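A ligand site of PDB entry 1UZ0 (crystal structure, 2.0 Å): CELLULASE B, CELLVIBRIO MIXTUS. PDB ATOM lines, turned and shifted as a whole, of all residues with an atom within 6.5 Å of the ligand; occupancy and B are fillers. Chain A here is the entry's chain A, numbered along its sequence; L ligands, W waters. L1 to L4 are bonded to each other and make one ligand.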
ATOM      1  N   SER A  12      28.629  20.457  34.739  1.00  0.00           N
ATOM      2  CA  SER A  12      27.753  21.572  34.326  1.00  0.00           C
ATOM      3  C   SER A  12      26.336  21.081  34.102  1.00  0.00           C
ATOM      4  O   SER A  12      25.372  21.831  34.276  1.00  0.00           O
ATOM      5  CB  SER A  12      28.302  22.288  33.074  1.00  0.00           C
ATOM      6  OG  SER A  12      28.515  21.417  31.956  1.00  0.00           O
ATOM      7  N   GLN A  13      26.221  19.809  33.707  1.00  0.00           N
ATOM      8  CA  GLN A  13      24.924  19.119  33.497  1.00  0.00           C
ATOM      9  C   GLN A  13      25.139  17.665  33.845  1.00  0.00           C
ATOM     10  O   GLN A  13      26.244  17.141  33.765  1.00  0.00           O
ATOM     11  CB  GLN A  13      24.380  19.257  32.059  1.00  0.00           C
ATOM     12  CG  GLN A  13      24.005  20.705  31.666  1.00  0.00           C
ATOM     13  CD  GLN A  13      25.202  21.556  31.078  1.00  0.00           C
ATOM     14  OE1 GLN A  13      26.242  21.016  30.649  1.00  0.00           O
ATOM     15  NE2 GLN A  13      25.011  22.903  31.054  1.00  0.00           N
ATOM     16  N   ALA A  36      23.364   2.458  34.631  1.00  0.00           N
ATOM     17  CA  ALA A  36      23.402   2.357  33.174  1.00  0.00           C
ATOM     18  C   ALA A  36      22.560   3.455  32.528  1.00  0.00           C
ATOM     19  O   ALA A  36      21.398   3.640  32.917  1.00  0.00           O
ATOM     20  CB  ALA A  36      22.890   0.997  32.713  1.00  0.00           C
ATOM     21  N   GLY A  37      23.172   4.176  31.586  1.00  0.00           N
ATOM     22  CA  GLY A  37      22.558   5.337  30.923  1.00  0.00           C
ATOM     23  C   GLY A  37      22.698   6.684  31.589  1.00  0.00           C
ATOM     24  O   GLY A  37      22.461   7.717  30.980  1.00  0.00           O
ATOM     25  N   ASP A  38      23.059   6.717  32.861  1.00  0.00           N
ATOM     26  CA  ASP A  38      23.377   7.997  33.520  1.00  0.00           C
ATOM     27  C   ASP A  38      24.605   8.647  32.887  1.00  0.00           C
ATOM     28  O   ASP A  38      25.457   7.990  32.261  1.00  0.00           O
ATOM     29  CB  ASP A  38      23.594   7.854  35.022  1.00  0.00           C
ATOM     30  CG  ASP A  38      22.346   7.391  35.763  1.00  0.00           C
ATOM     31  OD1 ASP A  38      21.215   7.528  35.251  1.00  0.00           O
ATOM     32  OD2 ASP A  38      22.416   6.920  36.906  1.00  0.00           O
ATOM     33  N   TRP A  39      24.737   9.955  33.078  1.00  0.00           N
ATOM     34  CA  TRP A  39      25.819  10.705  32.430  1.00  0.00           C
ATOM     35  C   TRP A  39      26.127  11.983  33.133  1.00  0.00           C
ATOM     36  O   TRP A  39      25.362  12.531  33.915  1.00  0.00           O
ATOM     37  CB  TRP A  39      25.532  10.919  30.929  1.00  0.00           C
ATOM     38  CG  TRP A  39      24.231  11.669  30.590  1.00  0.00           C
ATOM     39  CD1 TRP A  39      23.046  11.135  30.166  1.00  0.00           C
ATOM     40  CD2 TRP A  39      24.008  13.086  30.650  1.00  0.00           C
ATOM     41  NE1 TRP A  39      22.113  12.120  29.941  1.00  0.00           N
ATOM     42  CE2 TRP A  39      22.685  13.341  30.219  1.00  0.00           C
ATOM     43  CE3 TRP A  39      24.807  14.173  30.995  1.00  0.00           C
ATOM     44  CZ2 TRP A  39      22.120  14.615  30.183  1.00  0.00           C
ATOM     45  CZ3 TRP A  39      24.250  15.450  30.947  1.00  0.00           C
ATOM     46  CH2 TRP A  39      22.906  15.650  30.539  1.00  0.00           C
ATOM     47  N   LEU A  40      27.345  12.436  32.907  1.00  0.00           N
ATOM     48  CA  LEU A  40      27.868  13.659  33.457  1.00  0.00           C
ATOM     49  C   LEU A  40      28.483  14.454  32.312  1.00  0.00           C
ATOM     50  O   LEU A  40      29.196  13.900  31.468  1.00  0.00           O
ATOM     51  CB  LEU A  40      29.001  13.286  34.406  1.00  0.00           C
ATOM     52  CG  LEU A  40      28.591  12.425  35.570  1.00  0.00           C
ATOM     53  CD1 LEU A  40      29.837  11.690  36.129  1.00  0.00           C
ATOM     54  CD2 LEU A  40      27.943  13.296  36.631  1.00  0.00           C
ATOM     55  N   SER A  41      28.282  15.766  32.314  1.00  0.00           N
ATOM     56  CA  SER A  41      28.879  16.653  31.390  1.00  0.00           C
ATOM     57  C   SER A  41      29.764  17.696  32.039  1.00  0.00           C
ATOM     58  O   SER A  41      29.390  18.299  33.046  1.00  0.00           O
ATOM     59  CB  SER A  41      27.812  17.404  30.606  1.00  0.00           C
ATOM     60  OG  SER A  41      28.409  18.283  29.698  1.00  0.00           O
ATOM     61  N   TYR A  42      30.907  17.933  31.400  1.00  0.00           N
ATOM     62  CA  TYR A  42      31.839  18.975  31.809  1.00  0.00           C
ATOM     63  C   TYR A  42      31.987  20.057  30.745  1.00  0.00           C
ATOM     64  O   TYR A  42      33.024  20.775  30.699  1.00  0.00           O
ATOM     65  CB  TYR A  42      33.186  18.339  32.236  1.00  0.00           C
ATOM     66  CG  TYR A  42      32.930  17.340  33.288  1.00  0.00           C
ATOM     67  CD1 TYR A  42      32.707  15.994  32.967  1.00  0.00           C
ATOM     68  CD2 TYR A  42      32.865  17.720  34.641  1.00  0.00           C
ATOM     69  CE1 TYR A  42      32.404  15.051  33.952  1.00  0.00           C
ATOM     70  CE2 TYR A  42      32.530  16.785  35.651  1.00  0.00           C
ATOM     71  CZ  TYR A  42      32.329  15.448  35.295  1.00  0.00           C
ATOM     72  OH  TYR A  42      31.952  14.559  36.266  1.00  0.00           O
ATOM     73  N   ALA A  43      30.910  20.279  29.988  1.00  0.00           N
ATOM     74  CA  ALA A  43      30.915  21.259  28.872  1.00  0.00           C
ATOM     75  C   ALA A  43      31.162  22.692  29.345  1.00  0.00           C
ATOM     76  O   ALA A  43      31.772  23.495  28.632  1.00  0.00           O
ATOM     77  CB  ALA A  43      29.622  21.158  28.101  1.00  0.00           C
ATOM     78  N   GLY A  44      30.784  22.971  30.597  1.00  0.00           N
ATOM     79  CA  GLY A  44      30.947  24.270  31.255  1.00  0.00           C
ATOM     80  C   GLY A  44      32.388  24.609  31.600  1.00  0.00           C
ATOM     81  O   GLY A  44      32.672  25.754  31.869  1.00  0.00           O
ATOM     82  N   GLU A  73      33.988  10.515  26.619  1.00  0.00           N
ATOM     83  CA  GLU A  73      33.547  11.052  25.375  1.00  0.00           C
ATOM     84  C   GLU A  73      33.560  12.600  25.331  1.00  0.00           C
ATOM     85  O   GLU A  73      33.837  13.248  26.297  1.00  0.00           O
ATOM     86  CB  GLU A  73      32.139  10.511  25.065  1.00  0.00           C
ATOM     87  CG  GLU A  73      31.128  10.944  26.132  1.00  0.00           C
ATOM     88  CD  GLU A  73      29.769  10.270  26.051  1.00  0.00           C
ATOM     89  OE1 GLU A  73      29.694   9.083  25.688  1.00  0.00           O
ATOM     90  OE2 GLU A  73      28.744  10.949  26.337  1.00  0.00           O
ATOM     91  N   GLU A  74      33.241  13.147  24.169  1.00  0.00           N
ATOM     92  CA  GLU A  74      32.989  14.576  24.007  1.00  0.00           C
ATOM     93  C   GLU A  74      31.542  14.783  24.486  1.00  0.00           C
ATOM     94  O   GLU A  74      30.689  13.978  24.211  1.00  0.00           O
ATOM     95  CB  GLU A  74      33.184  14.908  22.513  1.00  0.00           C
ATOM     96  CG  GLU A  74      33.748  16.284  22.146  1.00  0.00           C
ATOM     97  CD  GLU A  74      35.067  16.670  22.762  1.00  0.00           C
ATOM     98  OE1 GLU A  74      35.921  15.814  23.171  1.00  0.00           O
ATOM     99  OE2 GLU A  74      35.211  17.923  22.824  1.00  0.00           O
ATOM    100  N   ALA A  75      31.300  15.856  25.234  1.00  0.00           N
ATOM    101  CA  ALA A  75      30.031  16.210  25.784  1.00  0.00           C
ATOM    102  C   ALA A  75      29.021  16.206  24.653  1.00  0.00           C
ATOM    103  O   ALA A  75      29.236  16.815  23.612  1.00  0.00           O
ATOM    104  CB  ALA A  75      30.095  17.554  26.416  1.00  0.00           C
ATOM    105  N   GLY A  76      27.957  15.459  24.854  1.00  0.00           N
ATOM    106  CA  GLY A  76      26.937  15.333  23.847  1.00  0.00           C
ATOM    107  C   GLY A  76      26.896  13.949  23.304  1.00  0.00           C
ATOM    108  O   GLY A  76      25.915  13.571  22.659  1.00  0.00           O
ATOM    109  N   GLY A  77      27.984  13.200  23.497  1.00  0.00           N
ATOM    110  CA  GLY A  77      28.048  11.815  23.083  1.00  0.00           C
ATOM    111  C   GLY A  77      28.835  11.414  21.854  1.00  0.00           C
ATOM    112  O   GLY A  77      28.937  10.205  21.574  1.00  0.00           O
ATOM    113  N   ALA A  78      29.457  12.347  21.159  1.00  0.00           N
ATOM    114  CA  ALA A  78      30.262  12.025  19.973  1.00  0.00           C
ATOM    115  C   ALA A  78      31.264  13.154  19.725  1.00  0.00           C
ATOM    116  O   ALA A  78      30.913  14.356  19.868  1.00  0.00           O
ATOM    117  CB  ALA A  78      29.313  11.891  18.723  1.00  0.00           C
ATOM    118  N   GLN A 110      35.190  19.686  25.179  1.00  0.00           N
ATOM    119  CA  GLN A 110      34.223  19.580  26.254  1.00  0.00           C
ATOM    120  C   GLN A 110      33.958  18.114  26.487  1.00  0.00           C
ATOM    121  O   GLN A 110      33.511  17.426  25.582  1.00  0.00           O
ATOM    122  CB  GLN A 110      32.956  20.354  25.875  1.00  0.00           C
ATOM    123  CG  GLN A 110      33.173  21.858  25.716  1.00  0.00           C
ATOM    124  CD  GLN A 110      31.975  22.555  25.083  1.00  0.00           C
ATOM    125  OE1 GLN A 110      31.667  22.286  23.943  1.00  0.00           O
ATOM    126  NE2 GLN A 110      31.281  23.440  25.850  1.00  0.00           N
ATOM    127  N   PHE A 111      34.311  17.613  27.666  1.00  0.00           N
ATOM    128  CA  PHE A 111      34.201  16.187  27.950  1.00  0.00           C
ATOM    129  C   PHE A 111      32.939  15.800  28.720  1.00  0.00           C
ATOM    130  O   PHE A 111      32.310  16.599  29.392  1.00  0.00           O
ATOM    131  CB  PHE A 111      35.438  15.740  28.738  1.00  0.00           C
ATOM    132  CG  PHE A 111      36.724  15.837  27.954  1.00  0.00           C
ATOM    133  CD1 PHE A 111      37.776  16.626  28.414  1.00  0.00           C
ATOM    134  CD2 PHE A 111      36.920  15.115  26.807  1.00  0.00           C
ATOM    135  CE1 PHE A 111      38.992  16.714  27.712  1.00  0.00           C
ATOM    136  CE2 PHE A 111      38.121  15.214  26.098  1.00  0.00           C
ATOM    137  CZ  PHE A 111      39.146  16.043  26.534  1.00  0.00           C
ATOM    138  N   GLY A 112      32.566  14.546  28.544  1.00  0.00           N
ATOM    139  CA  GLY A 112      31.455  13.923  29.182  1.00  0.00           C
ATOM    140  C   GLY A 112      31.845  12.489  29.537  1.00  0.00           C
ATOM    141  O   GLY A 112      32.809  11.933  29.002  1.00  0.00           O
ATOM    142  N   ILE A 113      31.080  11.918  30.439  1.00  0.00           N
ATOM    143  CA  ILE A 113      31.207  10.545  30.891  1.00  0.00           C
ATOM    144  C   ILE A 113      29.813   9.895  30.837  1.00  0.00           C
ATOM    145  O   ILE A 113      28.830  10.462  31.318  1.00  0.00           O
ATOM    146  CB  ILE A 113      31.785  10.522  32.280  1.00  0.00           C
ATOM    147  CG1 ILE A 113      33.262  10.948  32.230  1.00  0.00           C
ATOM    148  CG2 ILE A 113      31.677   9.124  32.875  1.00  0.00           C
ATOM    149  CD1 ILE A 113      33.831  11.214  33.547  1.00  0.00           C
ATOM    150  N   LYS A 114      29.740   8.717  30.236  1.00  0.00           N
ATOM    151  CA  LYS A 114      28.493   7.971  30.172  1.00  0.00           C
ATOM    152  C   LYS A 114      28.715   6.636  30.912  1.00  0.00           C
ATOM    153  O   LYS A 114      29.723   5.959  30.666  1.00  0.00           O
ATOM    154  CB  LYS A 114      28.158   7.751  28.691  1.00  0.00           C
ATOM    155  CG  LYS A 114      27.072   6.670  28.421  1.00  0.00           C
ATOM    156  CD  LYS A 114      25.700   7.172  28.850  1.00  0.00           C
ATOM    157  CE  LYS A 114      24.939   8.039  27.846  1.00  0.00           C
ATOM    158  NZ  LYS A 114      25.303   8.194  26.542  1.00  0.00           N
ATOM    159  N   ALA A 115      27.799   6.276  31.802  1.00  0.00           N
ATOM    160  CA  ALA A 115      27.773   4.999  32.441  1.00  0.00           C
ATOM    161  C   ALA A 115      27.119   3.933  31.539  1.00  0.00           C
ATOM    162  O   ALA A 115      25.915   3.997  31.218  1.00  0.00           O
ATOM    163  CB  ALA A 115      27.066   5.099  33.794  1.00  0.00           C
HETATM  164  C1  LIG L   1      25.260  19.062  28.093  1.00  0.00           C
HETATM  165  C2  LIG L   1      25.485  17.815  27.224  1.00  0.00           C
HETATM  166  C3  LIG L   1      24.183  17.010  27.169  1.00  0.00           C
HETATM  167  C4  LIG L   1      22.949  17.842  26.801  1.00  0.00           C
HETATM  168  C5  LIG L   1      21.624  17.011  26.922  1.00  0.00           C
HETATM  169  C6  LIG L   1      24.067  19.848  27.574  1.00  0.00           C
HETATM  170  O1  LIG L   1      23.842  20.874  28.493  1.00  0.00           O
HETATM  171  O2  LIG L   1      26.416  19.847  28.134  1.00  0.00           O
HETATM  172  O3  LIG L   1      26.562  17.029  27.746  1.00  0.00           O
HETATM  173  O4  LIG L   1      24.251  15.946  26.232  1.00  0.00           O
HETATM  174  O5  LIG L   1      22.877  19.038  27.573  1.00  0.00           O
HETATM  175  O6  LIG L   1      20.581  17.678  26.216  1.00  0.00           O
HETATM  176  C1  LG2 L   2      23.968  13.604  25.863  1.00  0.00           C
HETATM  177  C2  LG2 L   2      24.343  12.176  26.313  1.00  0.00           C
HETATM  178  C3  LG2 L   2      25.820  12.092  26.675  1.00  0.00           C
HETATM  179  C4  LG2 L   2      26.151  13.206  27.650  1.00  0.00           C
HETATM  180  C5  LG2 L   2      27.633  13.244  28.066  1.00  0.00           C
HETATM  181  C6  LG2 L   2      24.473  14.668  26.833  1.00  0.00           C
HETATM  182  O1  LG2 L   2      22.548  13.731  25.680  1.00  0.00           O
HETATM  183  O2  LG2 L   2      24.086  11.259  25.233  1.00  0.00           O
HETATM  184  O3  LG2 L   2      26.174  10.761  27.087  1.00  0.00           O
HETATM  185  O4  LG2 L   2      25.831  14.463  27.066  1.00  0.00           O
HETATM  186  O5  LG2 L   2      28.455  13.421  26.935  1.00  0.00           O
HETATM  187  C1  LG3 L   3      22.493   9.998  23.962  1.00  0.00           C
HETATM  188  C2  LG3 L   3      21.147   9.285  23.991  1.00  0.00           C
HETATM  189  C3  LG3 L   3      21.008   8.412  25.214  1.00  0.00           C
HETATM  190  C4  LG3 L   3      21.298   9.230  26.470  1.00  0.00           C
HETATM  191  C5  LG3 L   3      21.177   8.400  27.743  1.00  0.00           C
HETATM  192  C6  LG3 L   3      22.754  10.697  25.304  1.00  0.00           C
HETATM  193  O1  LG3 L   3      22.568  10.982  22.945  1.00  0.00           O
HETATM  194  O2  LG3 L   3      20.961   8.610  22.739  1.00  0.00           O
HETATM  195  O3  LG3 L   3      19.693   7.880  25.374  1.00  0.00           O
HETATM  196  O4  LG3 L   3      22.579   9.803  26.386  1.00  0.00           O
HETATM  197  O5  LG3 L   3      22.085   7.332  27.713  1.00  0.00           O
HETATM  198  C1  LG4 L   4      18.151   6.113  25.293  1.00  0.00           C
HETATM  199  C2  LG4 L   4      17.839   4.679  24.821  1.00  0.00           C
HETATM  200  C3  LG4 L   4      18.505   4.441  23.472  1.00  0.00           C
HETATM  201  C4  LG4 L   4      19.985   4.870  23.477  1.00  0.00           C
HETATM  202  C5  LG4 L   4      20.694   4.717  22.129  1.00  0.00           C
HETATM  203  C6  LG4 L   4      19.620   6.499  25.149  1.00  0.00           C
HETATM  204  O1  LG4 L   4      17.693   6.376  26.584  1.00  0.00           O
HETATM  205  O2  LG4 L   4      16.423   4.575  24.749  1.00  0.00           O
HETATM  206  O3  LG4 L   4      18.411   3.116  23.016  1.00  0.00           O
HETATM  207  O4  LG4 L   4      20.084   6.202  23.853  1.00  0.00           O
HETATM  208  O5  LG4 L   4      22.104   4.784  22.273  1.00  0.00           O
HETATM  209  O   HOH W   1      27.255  20.713  25.043  1.00  0.00           O
HETATM  210  O   HOH W   2      19.139   1.646  20.922  1.00  0.00           O
HETATM  211  O   HOH W   3      20.122  13.010  27.300  1.00  0.00           O
HETATM  212  O   HOH W   4      23.820   6.321  24.349  1.00  0.00           O
HETATM  213  O   HOH W   5      22.118   5.372  18.916  1.00  0.00           O
HETATM  214  O   HOH W   6      24.880  10.926  21.588  1.00  0.00           O
HETATM  215  O   HOH W   7      20.070  10.498  20.880  1.00  0.00           O
HETATM  216  O   HOH W   8      14.654   6.226  26.581  1.00  0.00           O
HETATM  217  O   HOH W   9      23.959   2.541  21.845  1.00  0.00           O
HETATM  218  O   HOH W  10      19.204  16.676  23.938  1.00  0.00           O
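N of Gly 77 is in hydrogen-bond range of O5 of LG2 L2 (3.5 Å).
An oxygen (O5) of LG2 L2 sits at hydrogen-bond distance from the side-chain carboxylate (OE2) of Glu 73, at 2.6 Å.
O of Gly 37 sits at hydrogen-bond distance from O5 of LG3 L3 (3.3 Å).
An oxygen (O2) of LIG L1 lies within hydrogen-bond range of the side-chain amide oxygen of Gln 13.
The side-chain hydroxyl (OG) of Ser 41 sits at hydrogen-bond distance from an oxygen (O3) of LIG L1 (3.0 Å).
The side-chain amino group of Lys 114 sits at hydrogen-bond distance from an oxygen (O3) of LG2 L2, 2.8 Å away.
An oxygen (O5) of LG2 L2 is in hydrogen-bond range of the backbone NH (N) of Gly 76.
OG of Ser 41 lies within hydrogen-bond range of N of Ala 43 (3.2 Å).
O of Ala 115 is in hydrogen-bond range of N of Gly 37.
The backbone carbonyl oxygen (O) of Leu 40 sits at hydrogen-bond distance from the backbone NH (N) of Ile 113 (2.9 Å).
O of Ala 43 sits at hydrogen-bond distance from NE2 of Gln 110 (2.8 Å).
The backbone NH (N) of Gln 110 lies within hydrogen-bond range of the side-chain carboxylate (OE2) of Glu 74, 2.9 Å away.
O of Gln 13 lies within hydrogen-bond range of N of Ser 41 (2.9 Å).
The backbone NH (N) of Ser 12 lies within hydrogen-bond range of the backbone carbonyl oxygen (O) of Ser 41 (2.8 Å).
The backbone carbonyl oxygen (O) of Gln 110 is in hydrogen-bond range of the backbone NH (N) of Ala 75 (2.7 Å).
Residues that only touch the ligand: Ala 75, Ala 43, Glu 74, Trp 39, Gly 112 and Leu 40.
Hydrophobic or aromatic side chains that line the ligand: Trp 39, Ala 43 and Ala 75.
Within 4 Å of the ligand: Gln 13, Gly 37, Trp 39, Leu 40, Ser 41, Ala 43, Glu 73, Glu 74, Ala 75, Gly 76, Gly 77, Gly 112 and Lys 114.
Water W6 bridges an oxygen (O1) of LG3 L3 (2.7 Å) and the backbone carbonyl oxygen of Gly 76 (3.0 Å).
Water W3 bridges O1 of LG2 L2 (3.0 Å) and NE1 of Trp 39 (3.4 Å).
Water W4 lies within hydrogen-bond range of an oxygen (O5) of LG4 L4 (3.1 Å) and the side-chain amino group of Lys 114 (3.2 Å).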
